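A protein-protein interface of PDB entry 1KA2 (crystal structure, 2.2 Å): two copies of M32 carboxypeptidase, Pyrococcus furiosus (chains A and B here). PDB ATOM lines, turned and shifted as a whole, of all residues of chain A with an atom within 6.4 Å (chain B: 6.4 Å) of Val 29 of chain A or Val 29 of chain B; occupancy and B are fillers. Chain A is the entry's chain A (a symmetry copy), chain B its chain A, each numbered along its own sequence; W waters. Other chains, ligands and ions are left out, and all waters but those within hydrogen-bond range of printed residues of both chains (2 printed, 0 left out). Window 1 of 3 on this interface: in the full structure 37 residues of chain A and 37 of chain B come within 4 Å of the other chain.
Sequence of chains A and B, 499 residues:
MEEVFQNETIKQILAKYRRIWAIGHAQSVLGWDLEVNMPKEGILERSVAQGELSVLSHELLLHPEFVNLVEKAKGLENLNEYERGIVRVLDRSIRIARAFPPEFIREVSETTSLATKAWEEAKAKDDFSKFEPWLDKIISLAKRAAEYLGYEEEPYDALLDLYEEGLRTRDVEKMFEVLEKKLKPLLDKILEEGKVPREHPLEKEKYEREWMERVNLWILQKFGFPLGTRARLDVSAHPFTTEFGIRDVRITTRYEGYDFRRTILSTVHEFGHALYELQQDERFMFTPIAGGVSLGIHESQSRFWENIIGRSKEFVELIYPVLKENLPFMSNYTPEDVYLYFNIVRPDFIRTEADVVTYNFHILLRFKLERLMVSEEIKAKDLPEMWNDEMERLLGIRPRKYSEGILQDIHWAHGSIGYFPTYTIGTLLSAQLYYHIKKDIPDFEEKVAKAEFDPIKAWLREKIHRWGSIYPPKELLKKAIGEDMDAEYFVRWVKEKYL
CG1 of Val 29 of chain A touches CG1 of Val 29 of chain B, 3.4 Å away. Val 29 of chain A touches Leu 30 of chain B (CB to CD1, 3.8 Å). Val 29 of chain A touches Arg 46 of chain B. Leu 30 of chain A touches Val 29 of chain B. CZ3 of Trp 32 of chain A touches OD2 of Asp 33 of chain B, at 3.7 Å. OD2 of Asp 33 of chain A touches CZ3 of Trp 32 of chain B, 3.7 Å away. Arg 46 of chain A touches Val 29 of chain B. Arg 46 of chain A touches Phe 244 of chain B. Phe 244 of chain A touches Arg 46 of chain B (CD1 to NH2, 3.4 Å).
His 25 of chain A touches Arg 46 of chain B, and with the chains exchanged Arg 46 of chain A touches His 25 of chain B. Trp 32 of chain A touches Asp 33 of chain B, and with the chains exchanged Asp 33 of chain A touches Trp 32 of chain B. Arg 46 of chain A touches Phe 244 of chain B, and with the chains exchanged Phe 244 of chain A touches Arg 46 of chain B. Arg 46 of chain A touches Asp 248 of chain B, and with the chains exchanged Asp 248 of chain A touches Arg 46 of chain B. 16 positions are printed for both chains. Of the 15 pairs that touch across the chains among the printed residues, 15 have their exchanged pair printed and touching as well.
Hydrophobic or aromatic side chains of chain B within 4 Å of the printed part of chain A: His 25, Val 29, Leu 30, Trp 32 and Phe 244. Along chain B the printed residues that touch a printed residue of chain A span positions 25 to 250. Along chain A the printed residues that touch a printed residue of chain B span positions 25 to 250. Among the printed residues, 15 pairs touch across the chains. Among the printed residues, Asp or Glu carboxylates within 4 Å of a Lys or Arg side-chain nitrogen of the other chain: Asp 33 of chain A with Arg 250 of chain B (2.8 Å), Arg 46 of chain A with Asp 248 of chain B (3.8 Å), Asp 248 of chain A with Arg 46 of chain B (3.8 Å) and Arg 250 of chain A with Asp 33 of chain B (2.8 Å).
NE2 of His 25 of chain B sits at hydrogen-bond distance from NE of Arg 46 of chain A. The side-chain carboxylate (OD2) of Asp 33 of chain B is in salt-bridge range of the guanidinium group (NH1) of Arg 250 of chain A, at 2.8 Å. NE2 of His 25 of chain A lies within hydrogen-bond range of NE of Arg 46 of chain B (2.7 Å). OD2 of Asp 248 of chain A lies within salt-bridge range of NH2 of Arg 46 of chain B (3.8 Å). The side-chain carboxylate (OD2) of Asp 248 of chain B lies within salt-bridge range of the guanidinium group (NH2) of Arg 46 of chain A, at 3.8 Å. The side-chain carboxylate (OD2) of Asp 33 of chain A is in salt-bridge range of the guanidinium group (NH1) of Arg 250 of chain B (2.8 Å).
Ser 28 of chain A touches none of the printed residues of chain B. Val 29 of chain A touches just these residues of chain B: Val 29, Leu 30 and Arg 46. Printed residues of chain B within 4 Å of Leu 30 of chain A: Val 29 (3.8 Å). Printed residues of chain B within 4 Å of Arg 46 of chain A: His 25 (2.7 Å), Val 29 (3.6 Å), Phe 244 (3.4 Å) and Asp 248 (3.8 Å). Of the printed residues of chain B, Asp 248 of chain A touches Arg 46 (3.8 Å). Of the printed residues of chain A, His 25 of chain B touches Arg 46. Of chain A, only Val 29, Leu 30 and Arg 46 come within 4 Å of Val 29 of chain B. Of the printed residues of chain A, Arg 46 of chain B touches His 25, Val 29, Phe 244 and Asp 248. The nearest residue of chain A that does not touch Val 29 of chain B is Asp 33 of chain A (4.5 Å).
Water W2 bridges the side-chain carboxylate (OD2) of Asp 248 of chain A and the guanidinium group (NH2) of Arg 46 of chain B. Water W1 lies within hydrogen-bond range of the side-chain carboxylate of Asp 248 of chain B (2.4 Å) and the guanidinium group of Arg 46 of chain A (3.2 Å).
ND1 of His 25 of chain B sits at hydrogen-bond distance from O of Phe 244 of chain B. NH1 of Arg 46 of chain B sits at hydrogen-bond distance from O of Leu 30 of chain B (3.0 Å). The side-chain carboxylate (OD1) of Asp 33 of chain B is in salt-bridge range of the guanidinium group (NH1) of Arg 46 of chain B. The guanidinium group (NE) of Arg 250 of chain B is in salt-bridge range of the side-chain carboxylate (OD1) of Asp 248 of chain B (2.9 Å). ND1 of His 25 of chain A lies within hydrogen-bond range of O of Phe 244 of chain A, 2.6 Å away. NH1 of Arg 46 of chain A sits at hydrogen-bond distance from O of Leu 30 of chain A (3.0 Å).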
ATOM      1  N   GLY A  24      15.868  14.910 -11.045  1.00  0.00           N
ATOM      2  CA  GLY A  24      16.180  15.028  -9.623  1.00  0.00           C
ATOM      3  C   GLY A  24      16.595  16.443  -9.240  1.00  0.00           C
ATOM      4  O   GLY A  24      16.223  16.964  -8.180  1.00  0.00           O
ATOM      5  N   HIS A  25      17.388  17.069 -10.100  1.00  0.00           N
ATOM      6  CA  HIS A  25      17.807  18.440  -9.863  1.00  0.00           C
ATOM      7  C   HIS A  25      16.516  19.235  -9.733  1.00  0.00           C
ATOM      8  O   HIS A  25      16.318  20.003  -8.795  1.00  0.00           O
ATOM      9  CB  HIS A  25      18.585  18.954 -11.062  1.00  0.00           C
ATOM     10  CG  HIS A  25      18.965  20.393 -10.957  1.00  0.00           C
ATOM     11  ND1 HIS A  25      20.003  20.832 -10.164  1.00  0.00           N
ATOM     12  CD2 HIS A  25      18.445  21.497 -11.545  1.00  0.00           C
ATOM     13  CE1 HIS A  25      20.108  22.146 -10.269  1.00  0.00           C
ATOM     14  NE2 HIS A  25      19.174  22.573 -11.102  1.00  0.00           N
ATOM     15  N   ALA A  26      15.627  19.020 -10.692  1.00  0.00           N
ATOM     16  CA  ALA A  26      14.344  19.706 -10.708  1.00  0.00           C
ATOM     17  C   ALA A  26      13.531  19.397  -9.440  1.00  0.00           C
ATOM     18  O   ALA A  26      12.977  20.301  -8.836  1.00  0.00           O
ATOM     19  CB  ALA A  26      13.567  19.313 -11.961  1.00  0.00           C
ATOM     20  N   GLN A  27      13.476  18.135  -9.019  1.00  0.00           N
ATOM     21  CA  GLN A  27      12.714  17.798  -7.808  1.00  0.00           C
ATOM     22  C   GLN A  27      13.224  18.557  -6.582  1.00  0.00           C
ATOM     23  O   GLN A  27      12.434  19.032  -5.770  1.00  0.00           O
ATOM     24  CB  GLN A  27      12.754  16.281  -7.531  1.00  0.00           C
ATOM     25  CG  GLN A  27      11.902  15.417  -8.461  1.00  0.00           C
ATOM     26  CD  GLN A  27      10.413  15.418  -8.116  1.00  0.00           C
ATOM     27  OE1 GLN A  27       9.731  14.394  -8.247  1.00  0.00           O
ATOM     28  NE2 GLN A  27       9.903  16.564  -7.688  1.00  0.00           N
ATOM     29  N   SER A  28      14.541  18.676  -6.444  1.00  0.00           N
ATOM     30  CA  SER A  28      15.131  19.389  -5.305  1.00  0.00           C
ATOM     31  C   SER A  28      14.726  20.856  -5.290  1.00  0.00           C
ATOM     32  O   SER A  28      14.352  21.416  -4.248  1.00  0.00           O
ATOM     33  CB  SER A  28      16.659  19.308  -5.353  1.00  0.00           C
ATOM     34  OG  SER A  28      17.110  17.974  -5.229  1.00  0.00           O
ATOM     35  N   VAL A  29      14.823  21.487  -6.451  1.00  0.00           N
ATOM     36  CA  VAL A  29      14.466  22.886  -6.564  1.00  0.00           C
ATOM     37  C   VAL A  29      12.999  23.075  -6.192  1.00  0.00           C
ATOM     38  O   VAL A  29      12.650  24.019  -5.497  1.00  0.00           O
ATOM     39  CB  VAL A  29      14.734  23.403  -7.992  1.00  0.00           C
ATOM     40  CG1 VAL A  29      14.260  24.835  -8.126  1.00  0.00           C
ATOM     41  CG2 VAL A  29      16.233  23.335  -8.270  1.00  0.00           C
ATOM     42  N   LEU A  30      12.155  22.157  -6.643  1.00  0.00           N
ATOM     43  CA  LEU A  30      10.723  22.198  -6.354  1.00  0.00           C
ATOM     44  C   LEU A  30      10.442  22.105  -4.863  1.00  0.00           C
ATOM     45  O   LEU A  30       9.692  22.911  -4.314  1.00  0.00           O
ATOM     46  CB  LEU A  30      10.021  21.048  -7.084  1.00  0.00           C
ATOM     47  CG  LEU A  30       9.298  21.384  -8.387  1.00  0.00           C
ATOM     48  CD1 LEU A  30       9.977  22.521  -9.092  1.00  0.00           C
ATOM     49  CD2 LEU A  30       9.228  20.138  -9.265  1.00  0.00           C
ATOM     50  N   GLY A  31      11.045  21.109  -4.211  1.00  0.00           N
ATOM     51  CA  GLY A  31      10.849  20.921  -2.785  1.00  0.00           C
ATOM     52  C   GLY A  31      11.385  22.076  -1.977  1.00  0.00           C
ATOM     53  O   GLY A  31      10.718  22.577  -1.068  1.00  0.00           O
ATOM     54  N   TRP A  32      12.594  22.514  -2.303  1.00  0.00           N
ATOM     55  CA  TRP A  32      13.185  23.639  -1.594  1.00  0.00           C
ATOM     56  C   TRP A  32      12.286  24.862  -1.721  1.00  0.00           C
ATOM     57  O   TRP A  32      11.955  25.520  -0.732  1.00  0.00           O
ATOM     58  CB  TRP A  32      14.574  23.963  -2.177  1.00  0.00           C
ATOM     59  CG  TRP A  32      15.241  25.165  -1.567  1.00  0.00           C
ATOM     60  CD1 TRP A  32      15.943  25.210  -0.399  1.00  0.00           C
ATOM     61  CD2 TRP A  32      15.243  26.503  -2.090  1.00  0.00           C
ATOM     62  NE1 TRP A  32      16.380  26.492  -0.158  1.00  0.00           N
ATOM     63  CE2 TRP A  32      15.964  27.304  -1.183  1.00  0.00           C
ATOM     64  CE3 TRP A  32      14.699  27.099  -3.243  1.00  0.00           C
ATOM     65  CZ2 TRP A  32      16.162  28.681  -1.386  1.00  0.00           C
ATOM     66  CZ3 TRP A  32      14.893  28.468  -3.447  1.00  0.00           C
ATOM     67  CH2 TRP A  32      15.619  29.244  -2.524  1.00  0.00           C
ATOM     68  N   ASP A  33      11.890  25.171  -2.952  1.00  0.00           N
ATOM     69  CA  ASP A  33      11.061  26.348  -3.190  1.00  0.00           C
ATOM     70  C   ASP A  33       9.720  26.222  -2.478  1.00  0.00           C
ATOM     71  O   ASP A  33       9.204  27.195  -1.924  1.00  0.00           O
ATOM     72  CB  ASP A  33      10.858  26.566  -4.700  1.00  0.00           C
ATOM     73  CG  ASP A  33       9.885  27.681  -4.990  1.00  0.00           C
ATOM     74  OD1 ASP A  33       8.691  27.392  -5.227  1.00  0.00           O
ATOM     75  OD2 ASP A  33      10.315  28.849  -4.946  1.00  0.00           O
ATOM     76  N   LEU A  34       9.157  25.020  -2.485  1.00  0.00           N
ATOM     77  CA  LEU A  34       7.892  24.806  -1.802  1.00  0.00           C
ATOM     78  C   LEU A  34       8.014  25.254  -0.341  1.00  0.00           C
ATOM     79  O   LEU A  34       7.139  25.958   0.160  1.00  0.00           O
ATOM     80  CB  LEU A  34       7.481  23.331  -1.914  1.00  0.00           C
ATOM     81  CG  LEU A  34       6.539  22.643  -0.910  1.00  0.00           C
ATOM     82  CD1 LEU A  34       5.562  23.591  -0.282  1.00  0.00           C
ATOM     83  CD2 LEU A  34       5.814  21.528  -1.643  1.00  0.00           C
ATOM     84  N   ARG A  46       2.055  22.628  -7.470  1.00  0.00           N
ATOM     85  CA  ARG A  46       3.393  22.151  -7.153  1.00  0.00           C
ATOM     86  C   ARG A  46       3.315  20.636  -6.938  1.00  0.00           C
ATOM     87  O   ARG A  46       4.117  19.883  -7.498  1.00  0.00           O
ATOM     88  CB  ARG A  46       3.920  22.842  -5.889  1.00  0.00           C
ATOM     89  CG  ARG A  46       5.319  22.385  -5.416  1.00  0.00           C
ATOM     90  CD  ARG A  46       6.356  22.425  -6.539  1.00  0.00           C
ATOM     91  NE  ARG A  46       6.361  23.734  -7.171  1.00  0.00           N
ATOM     92  CZ  ARG A  46       6.984  24.807  -6.699  1.00  0.00           C
ATOM     93  NH1 ARG A  46       7.690  24.736  -5.576  1.00  0.00           N
ATOM     94  NH2 ARG A  46       6.858  25.968  -7.332  1.00  0.00           N
ATOM     95  N   THR A 242      19.627  20.861   1.115  1.00  0.00           N
ATOM     96  CA  THR A 242      19.359  20.320  -0.213  1.00  0.00           C
ATOM     97  C   THR A 242      20.564  20.506  -1.092  1.00  0.00           C
ATOM     98  O   THR A 242      21.319  21.457  -0.934  1.00  0.00           O
ATOM     99  CB  THR A 242      18.258  21.039  -0.986  1.00  0.00           C
ATOM    100  OG1 THR A 242      17.726  22.116  -0.208  1.00  0.00           O
ATOM    101  CG2 THR A 242      17.207  20.050  -1.421  1.00  0.00           C
ATOM    102  N   PHE A 244      21.311  20.958  -5.011  1.00  0.00           N
ATOM    103  CA  PHE A 244      20.819  21.124  -6.371  1.00  0.00           C
ATOM    104  C   PHE A 244      21.986  20.627  -7.234  1.00  0.00           C
ATOM    105  O   PHE A 244      21.812  20.176  -8.365  1.00  0.00           O
ATOM    106  CB  PHE A 244      20.531  22.603  -6.674  1.00  0.00           C
ATOM    107  CG  PHE A 244      19.322  23.167  -5.959  1.00  0.00           C
ATOM    108  CD1 PHE A 244      18.937  24.486  -6.172  1.00  0.00           C
ATOM    109  CD2 PHE A 244      18.587  22.395  -5.057  1.00  0.00           C
ATOM    110  CE1 PHE A 244      17.840  25.040  -5.501  1.00  0.00           C
ATOM    111  CE2 PHE A 244      17.478  22.945  -4.373  1.00  0.00           C
ATOM    112  CZ  PHE A 244      17.113  24.273  -4.602  1.00  0.00           C
ATOM    113  N   ASP A 248      26.001  24.000  -5.788  1.00  0.00           N
ATOM    114  CA  ASP A 248      24.772  24.678  -5.385  1.00  0.00           C
ATOM    115  C   ASP A 248      24.115  23.880  -4.267  1.00  0.00           C
ATOM    116  O   ASP A 248      23.303  23.003  -4.534  1.00  0.00           O
ATOM    117  CB  ASP A 248      23.808  24.796  -6.578  1.00  0.00           C
ATOM    118  CG  ASP A 248      22.647  25.735  -6.304  1.00  0.00           C
ATOM    119  OD1 ASP A 248      22.496  26.183  -5.151  1.00  0.00           O
ATOM    120  OD2 ASP A 248      21.873  26.033  -7.246  1.00  0.00           O
ATOM    121  N   ARG A 250      22.060  24.214  -0.504  1.00  0.00           N
ATOM    122  CA  ARG A 250      21.336  25.149   0.332  1.00  0.00           C
ATOM    123  C   ARG A 250      20.808  24.590   1.646  1.00  0.00           C
ATOM    124  O   ARG A 250      20.380  23.437   1.722  1.00  0.00           O
ATOM    125  CB  ARG A 250      20.184  25.721  -0.487  1.00  0.00           C
ATOM    126  CG  ARG A 250      20.639  26.191  -1.862  1.00  0.00           C
ATOM    127  CD  ARG A 250      19.548  26.901  -2.655  1.00  0.00           C
ATOM    128  NE  ARG A 250      19.981  27.141  -4.026  1.00  0.00           N
ATOM    129  CZ  ARG A 250      19.220  27.688  -4.971  1.00  0.00           C
ATOM    130  NH1 ARG A 250      17.966  28.060  -4.704  1.00  0.00           N
ATOM    131  NH2 ARG A 250      19.720  27.868  -6.188  1.00  0.00           N
ATOM    132  N   GLY B  24       7.303  21.516 -17.659  1.00  0.00           N
ATOM    133  CA  GLY B  24       7.245  22.963 -17.848  1.00  0.00           C
ATOM    134  C   GLY B  24       7.183  23.714 -16.524  1.00  0.00           C
ATOM    135  O   GLY B  24       7.811  24.766 -16.345  1.00  0.00           O
ATOM    136  N   HIS B  25       6.406  23.182 -15.590  1.00  0.00           N
ATOM    137  CA  HIS B  25       6.308  23.786 -14.272  1.00  0.00           C
ATOM    138  C   HIS B  25       7.735  23.825 -13.744  1.00  0.00           C
ATOM    139  O   HIS B  25       8.224  24.847 -13.272  1.00  0.00           O
ATOM    140  CB  HIS B  25       5.469  22.903 -13.364  1.00  0.00           C
ATOM    141  CG  HIS B  25       5.403  23.386 -11.953  1.00  0.00           C
ATOM    142  ND1 HIS B  25       4.608  24.444 -11.568  1.00  0.00           N
ATOM    143  CD2 HIS B  25       6.032  22.958 -10.834  1.00  0.00           C
ATOM    144  CE1 HIS B  25       4.750  24.646 -10.268  1.00  0.00           C
ATOM    145  NE2 HIS B  25       5.609  23.756  -9.800  1.00  0.00           N
ATOM    146  N   ALA B  26       8.404  22.686 -13.852  1.00  0.00           N
ATOM    147  CA  ALA B  26       9.778  22.564 -13.392  1.00  0.00           C
ATOM    148  C   ALA B  26      10.701  23.550 -14.126  1.00  0.00           C
ATOM    149  O   ALA B  26      11.511  24.211 -13.497  1.00  0.00           O
ATOM    150  CB  ALA B  26      10.257  21.127 -13.580  1.00  0.00           C
ATOM    151  N   GLN B  27      10.571  23.672 -15.446  1.00  0.00           N
ATOM    152  CA  GLN B  27      11.430  24.607 -16.186  1.00  0.00           C
ATOM    153  C   GLN B  27      11.278  26.043 -15.682  1.00  0.00           C
ATOM    154  O   GLN B  27      12.262  26.766 -15.551  1.00  0.00           O
ATOM    155  CB  GLN B  27      11.135  24.555 -17.699  1.00  0.00           C
ATOM    156  CG  GLN B  27      11.644  23.312 -18.428  1.00  0.00           C
ATOM    157  CD  GLN B  27      13.139  23.348 -18.744  1.00  0.00           C
ATOM    158  OE1 GLN B  27      13.576  22.869 -19.798  1.00  0.00           O
ATOM    159  NE2 GLN B  27      13.926  23.901 -17.833  1.00  0.00           N
ATOM    160  N   SER B  28      10.048  26.461 -15.397  1.00  0.00           N
ATOM    161  CA  SER B  28       9.795  27.820 -14.903  1.00  0.00           C
ATOM    162  C   SER B  28      10.480  28.069 -13.567  1.00  0.00           C
ATOM    163  O   SER B  28      11.114  29.111 -13.347  1.00  0.00           O
ATOM    164  CB  SER B  28       8.293  28.059 -14.731  1.00  0.00           C
ATOM    165  OG  SER B  28       7.612  27.981 -15.968  1.00  0.00           O
ATOM    166  N   VAL B  29      10.330  27.112 -12.662  1.00  0.00           N
ATOM    167  CA  VAL B  29      10.934  27.233 -11.352  1.00  0.00           C
ATOM    168  C   VAL B  29      12.449  27.340 -11.491  1.00  0.00           C
ATOM    169  O   VAL B  29      13.082  28.138 -10.814  1.00  0.00           O
ATOM    170  CB  VAL B  29      10.555  26.030 -10.464  1.00  0.00           C
ATOM    171  CG1 VAL B  29      11.275  26.116  -9.135  1.00  0.00           C
ATOM    172  CG2 VAL B  29       9.047  26.046 -10.226  1.00  0.00           C
ATOM    173  N   LEU B  30      13.014  26.544 -12.390  1.00  0.00           N
ATOM    174  CA  LEU B  30      14.454  26.546 -12.645  1.00  0.00           C
ATOM    175  C   LEU B  30      14.939  27.897 -13.145  1.00  0.00           C
ATOM    176  O   LEU B  30      15.910  28.447 -12.626  1.00  0.00           O
ATOM    177  CB  LEU B  30      14.791  25.463 -13.674  1.00  0.00           C
ATOM    178  CG  LEU B  30      15.355  24.146 -13.144  1.00  0.00           C
ATOM    179  CD1 LEU B  30      14.812  23.850 -11.777  1.00  0.00           C
ATOM    180  CD2 LEU B  30      15.040  23.026 -14.131  1.00  0.00           C
ATOM    181  N   GLY B  31      14.260  28.427 -14.164  1.00  0.00           N
ATOM    182  CA  GLY B  31      14.635  29.712 -14.726  1.00  0.00           C
ATOM    183  C   GLY B  31      14.471  30.838 -13.736  1.00  0.00           C
ATOM    184  O   GLY B  31      15.356  31.683 -13.585  1.00  0.00           O
ATOM    185  N   TRP B  32      13.336  30.860 -13.049  1.00  0.00           N
ATOM    186  CA  TRP B  32      13.097  31.895 -12.056  1.00  0.00           C
ATOM    187  C   TRP B  32      14.189  31.858 -10.994  1.00  0.00           C
ATOM    188  O   TRP B  32      14.793  32.879 -10.660  1.00  0.00           O
ATOM    189  CB  TRP B  32      11.726  31.682 -11.386  1.00  0.00           C
ATOM    190  CG  TRP B  32      11.412  32.655 -10.282  1.00  0.00           C
ATOM    191  CD1 TRP B  32      10.924  33.920 -10.417  1.00  0.00           C
ATOM    192  CD2 TRP B  32      11.594  32.441  -8.873  1.00  0.00           C
ATOM    193  NE1 TRP B  32      10.792  34.512  -9.183  1.00  0.00           N
ATOM    194  CE2 TRP B  32      11.196  33.623  -8.218  1.00  0.00           C
ATOM    195  CE3 TRP B  32      12.058  31.359  -8.104  1.00  0.00           C
ATOM    196  CZ2 TRP B  32      11.245  33.763  -6.820  1.00  0.00           C
ATOM    197  CZ3 TRP B  32      12.110  31.494  -6.713  1.00  0.00           C
ATOM    198  CH2 TRP B  32      11.704  32.688  -6.085  1.00  0.00           C
ATOM    199  N   ASP B  33      14.441  30.668 -10.457  1.00  0.00           N
ATOM    200  CA  ASP B  33      15.439  30.529  -9.402  1.00  0.00           C
ATOM    201  C   ASP B  33      16.823  30.918  -9.906  1.00  0.00           C
ATOM    202  O   ASP B  33      17.601  31.555  -9.192  1.00  0.00           O
ATOM    203  CB  ASP B  33      15.444  29.091  -8.853  1.00  0.00           C
ATOM    204  CG  ASP B  33      16.561  28.860  -7.866  1.00  0.00           C
ATOM    205  OD1 ASP B  33      17.622  28.335  -8.271  1.00  0.00           O
ATOM    206  OD2 ASP B  33      16.382  29.238  -6.693  1.00  0.00           O
ATOM    207  N   LEU B  34      17.130  30.542 -11.142  1.00  0.00           N
ATOM    208  CA  LEU B  34      18.417  30.900 -11.712  1.00  0.00           C
ATOM    209  C   LEU B  34      18.616  32.418 -11.624  1.00  0.00           C
ATOM    210  O   LEU B  34      19.680  32.875 -11.211  1.00  0.00           O
ATOM    211  CB  LEU B  34      18.506  30.396 -13.160  1.00  0.00           C
ATOM    212  CG  LEU B  34      19.438  31.022 -14.212  1.00  0.00           C
ATOM    213  CD1 LEU B  34      20.669  31.633 -13.612  1.00  0.00           C
ATOM    214  CD2 LEU B  34      19.805  29.939 -15.211  1.00  0.00           C
ATOM    215  N   ARG B  46      22.754  23.857 -13.309  1.00  0.00           N
ATOM    216  CA  ARG B  46      21.414  24.323 -13.634  1.00  0.00           C
ATOM    217  C   ARG B  46      21.223  24.189 -15.148  1.00  0.00           C
ATOM    218  O   ARG B  46      20.211  23.651 -15.607  1.00  0.00           O
ATOM    219  CB  ARG B  46      21.237  25.784 -13.203  1.00  0.00           C
ATOM    220  CG  ARG B  46      19.866  26.416 -13.539  1.00  0.00           C
ATOM    221  CD  ARG B  46      18.696  25.555 -13.062  1.00  0.00           C
ATOM    222  NE  ARG B  46      18.851  25.232 -11.654  1.00  0.00           N
ATOM    223  CZ  ARG B  46      18.534  26.036 -10.646  1.00  0.00           C
ATOM    224  NH1 ARG B  46      18.012  27.235 -10.881  1.00  0.00           N
ATOM    225  NH2 ARG B  46      18.787  25.655  -9.399  1.00  0.00           N
ATOM    226  N   THR B 242       6.734  35.166 -14.377  1.00  0.00           N
ATOM    227  CA  THR B 242       6.681  33.726 -14.609  1.00  0.00           C
ATOM    228  C   THR B 242       5.414  33.164 -14.026  1.00  0.00           C
ATOM    229  O   THR B 242       4.896  33.668 -13.039  1.00  0.00           O
ATOM    230  CB  THR B 242       7.767  32.923 -13.903  1.00  0.00           C
ATOM    231  OG1 THR B 242       8.616  33.793 -13.146  1.00  0.00           O
ATOM    232  CG2 THR B 242       8.522  32.087 -14.905  1.00  0.00           C
ATOM    233  N   PHE B 244       4.170  29.659 -12.513  1.00  0.00           N
ATOM    234  CA  PHE B 244       4.467  28.296 -12.095  1.00  0.00           C
ATOM    235  C   PHE B 244       3.105  27.595 -12.177  1.00  0.00           C
ATOM    236  O   PHE B 244       3.008  26.382 -12.356  1.00  0.00           O
ATOM    237  CB  PHE B 244       4.991  28.266 -10.650  1.00  0.00           C
ATOM    238  CG  PHE B 244       6.384  28.832 -10.476  1.00  0.00           C
ATOM    239  CD1 PHE B 244       6.985  28.835  -9.221  1.00  0.00           C
ATOM    240  CD2 PHE B 244       7.084  29.384 -11.550  1.00  0.00           C
ATOM    241  CE1 PHE B 244       8.260  29.378  -9.028  1.00  0.00           C
ATOM    242  CE2 PHE B 244       8.372  29.937 -11.366  1.00  0.00           C
ATOM    243  CZ  PHE B 244       8.952  29.930 -10.096  1.00  0.00           C
ATOM    244  N   ASP B 248       0.112  30.494  -8.681  1.00  0.00           N
ATOM    245  CA  ASP B 248       1.498  30.783  -8.323  1.00  0.00           C
ATOM    246  C   ASP B 248       2.150  31.551  -9.464  1.00  0.00           C
ATOM    247  O   ASP B 248       2.721  30.947 -10.363  1.00  0.00           O
ATOM    248  CB  ASP B 248       2.268  29.476  -8.066  1.00  0.00           C
ATOM    249  CG  ASP B 248       3.620  29.709  -7.416  1.00  0.00           C
ATOM    250  OD1 ASP B 248       4.034  30.878  -7.295  1.00  0.00           O
ATOM    251  OD2 ASP B 248       4.281  28.719  -7.020  1.00  0.00           O
ATOM    252  N   ARG B 250       4.790  34.815 -10.392  1.00  0.00           N
ATOM    253  CA  ARG B 250       5.806  35.672  -9.816  1.00  0.00           C
ATOM    254  C   ARG B 250       6.412  36.705 -10.757  1.00  0.00           C
ATOM    255  O   ARG B 250       6.610  36.446 -11.945  1.00  0.00           O
ATOM    256  CB  ARG B 250       6.907  34.784  -9.246  1.00  0.00           C
ATOM    257  CG  ARG B 250       6.346  33.659  -8.387  1.00  0.00           C
ATOM    258  CD  ARG B 250       7.419  32.837  -7.682  1.00  0.00           C
ATOM    259  NE  ARG B 250       6.833  31.662  -7.048  1.00  0.00           N
ATOM    260  CZ  ARG B 250       7.530  30.726  -6.410  1.00  0.00           C
ATOM    261  NH1 ARG B 250       8.859  30.812  -6.315  1.00  0.00           N
ATOM    262  NH2 ARG B 250       6.893  29.698  -5.861  1.00  0.00           N
HETATM  263  O   HOH W   1       3.697  26.410  -7.424  1.00  0.00           O
HETATM  264  O   HOH W   2      21.919  25.036  -9.446  1.00  0.00           O
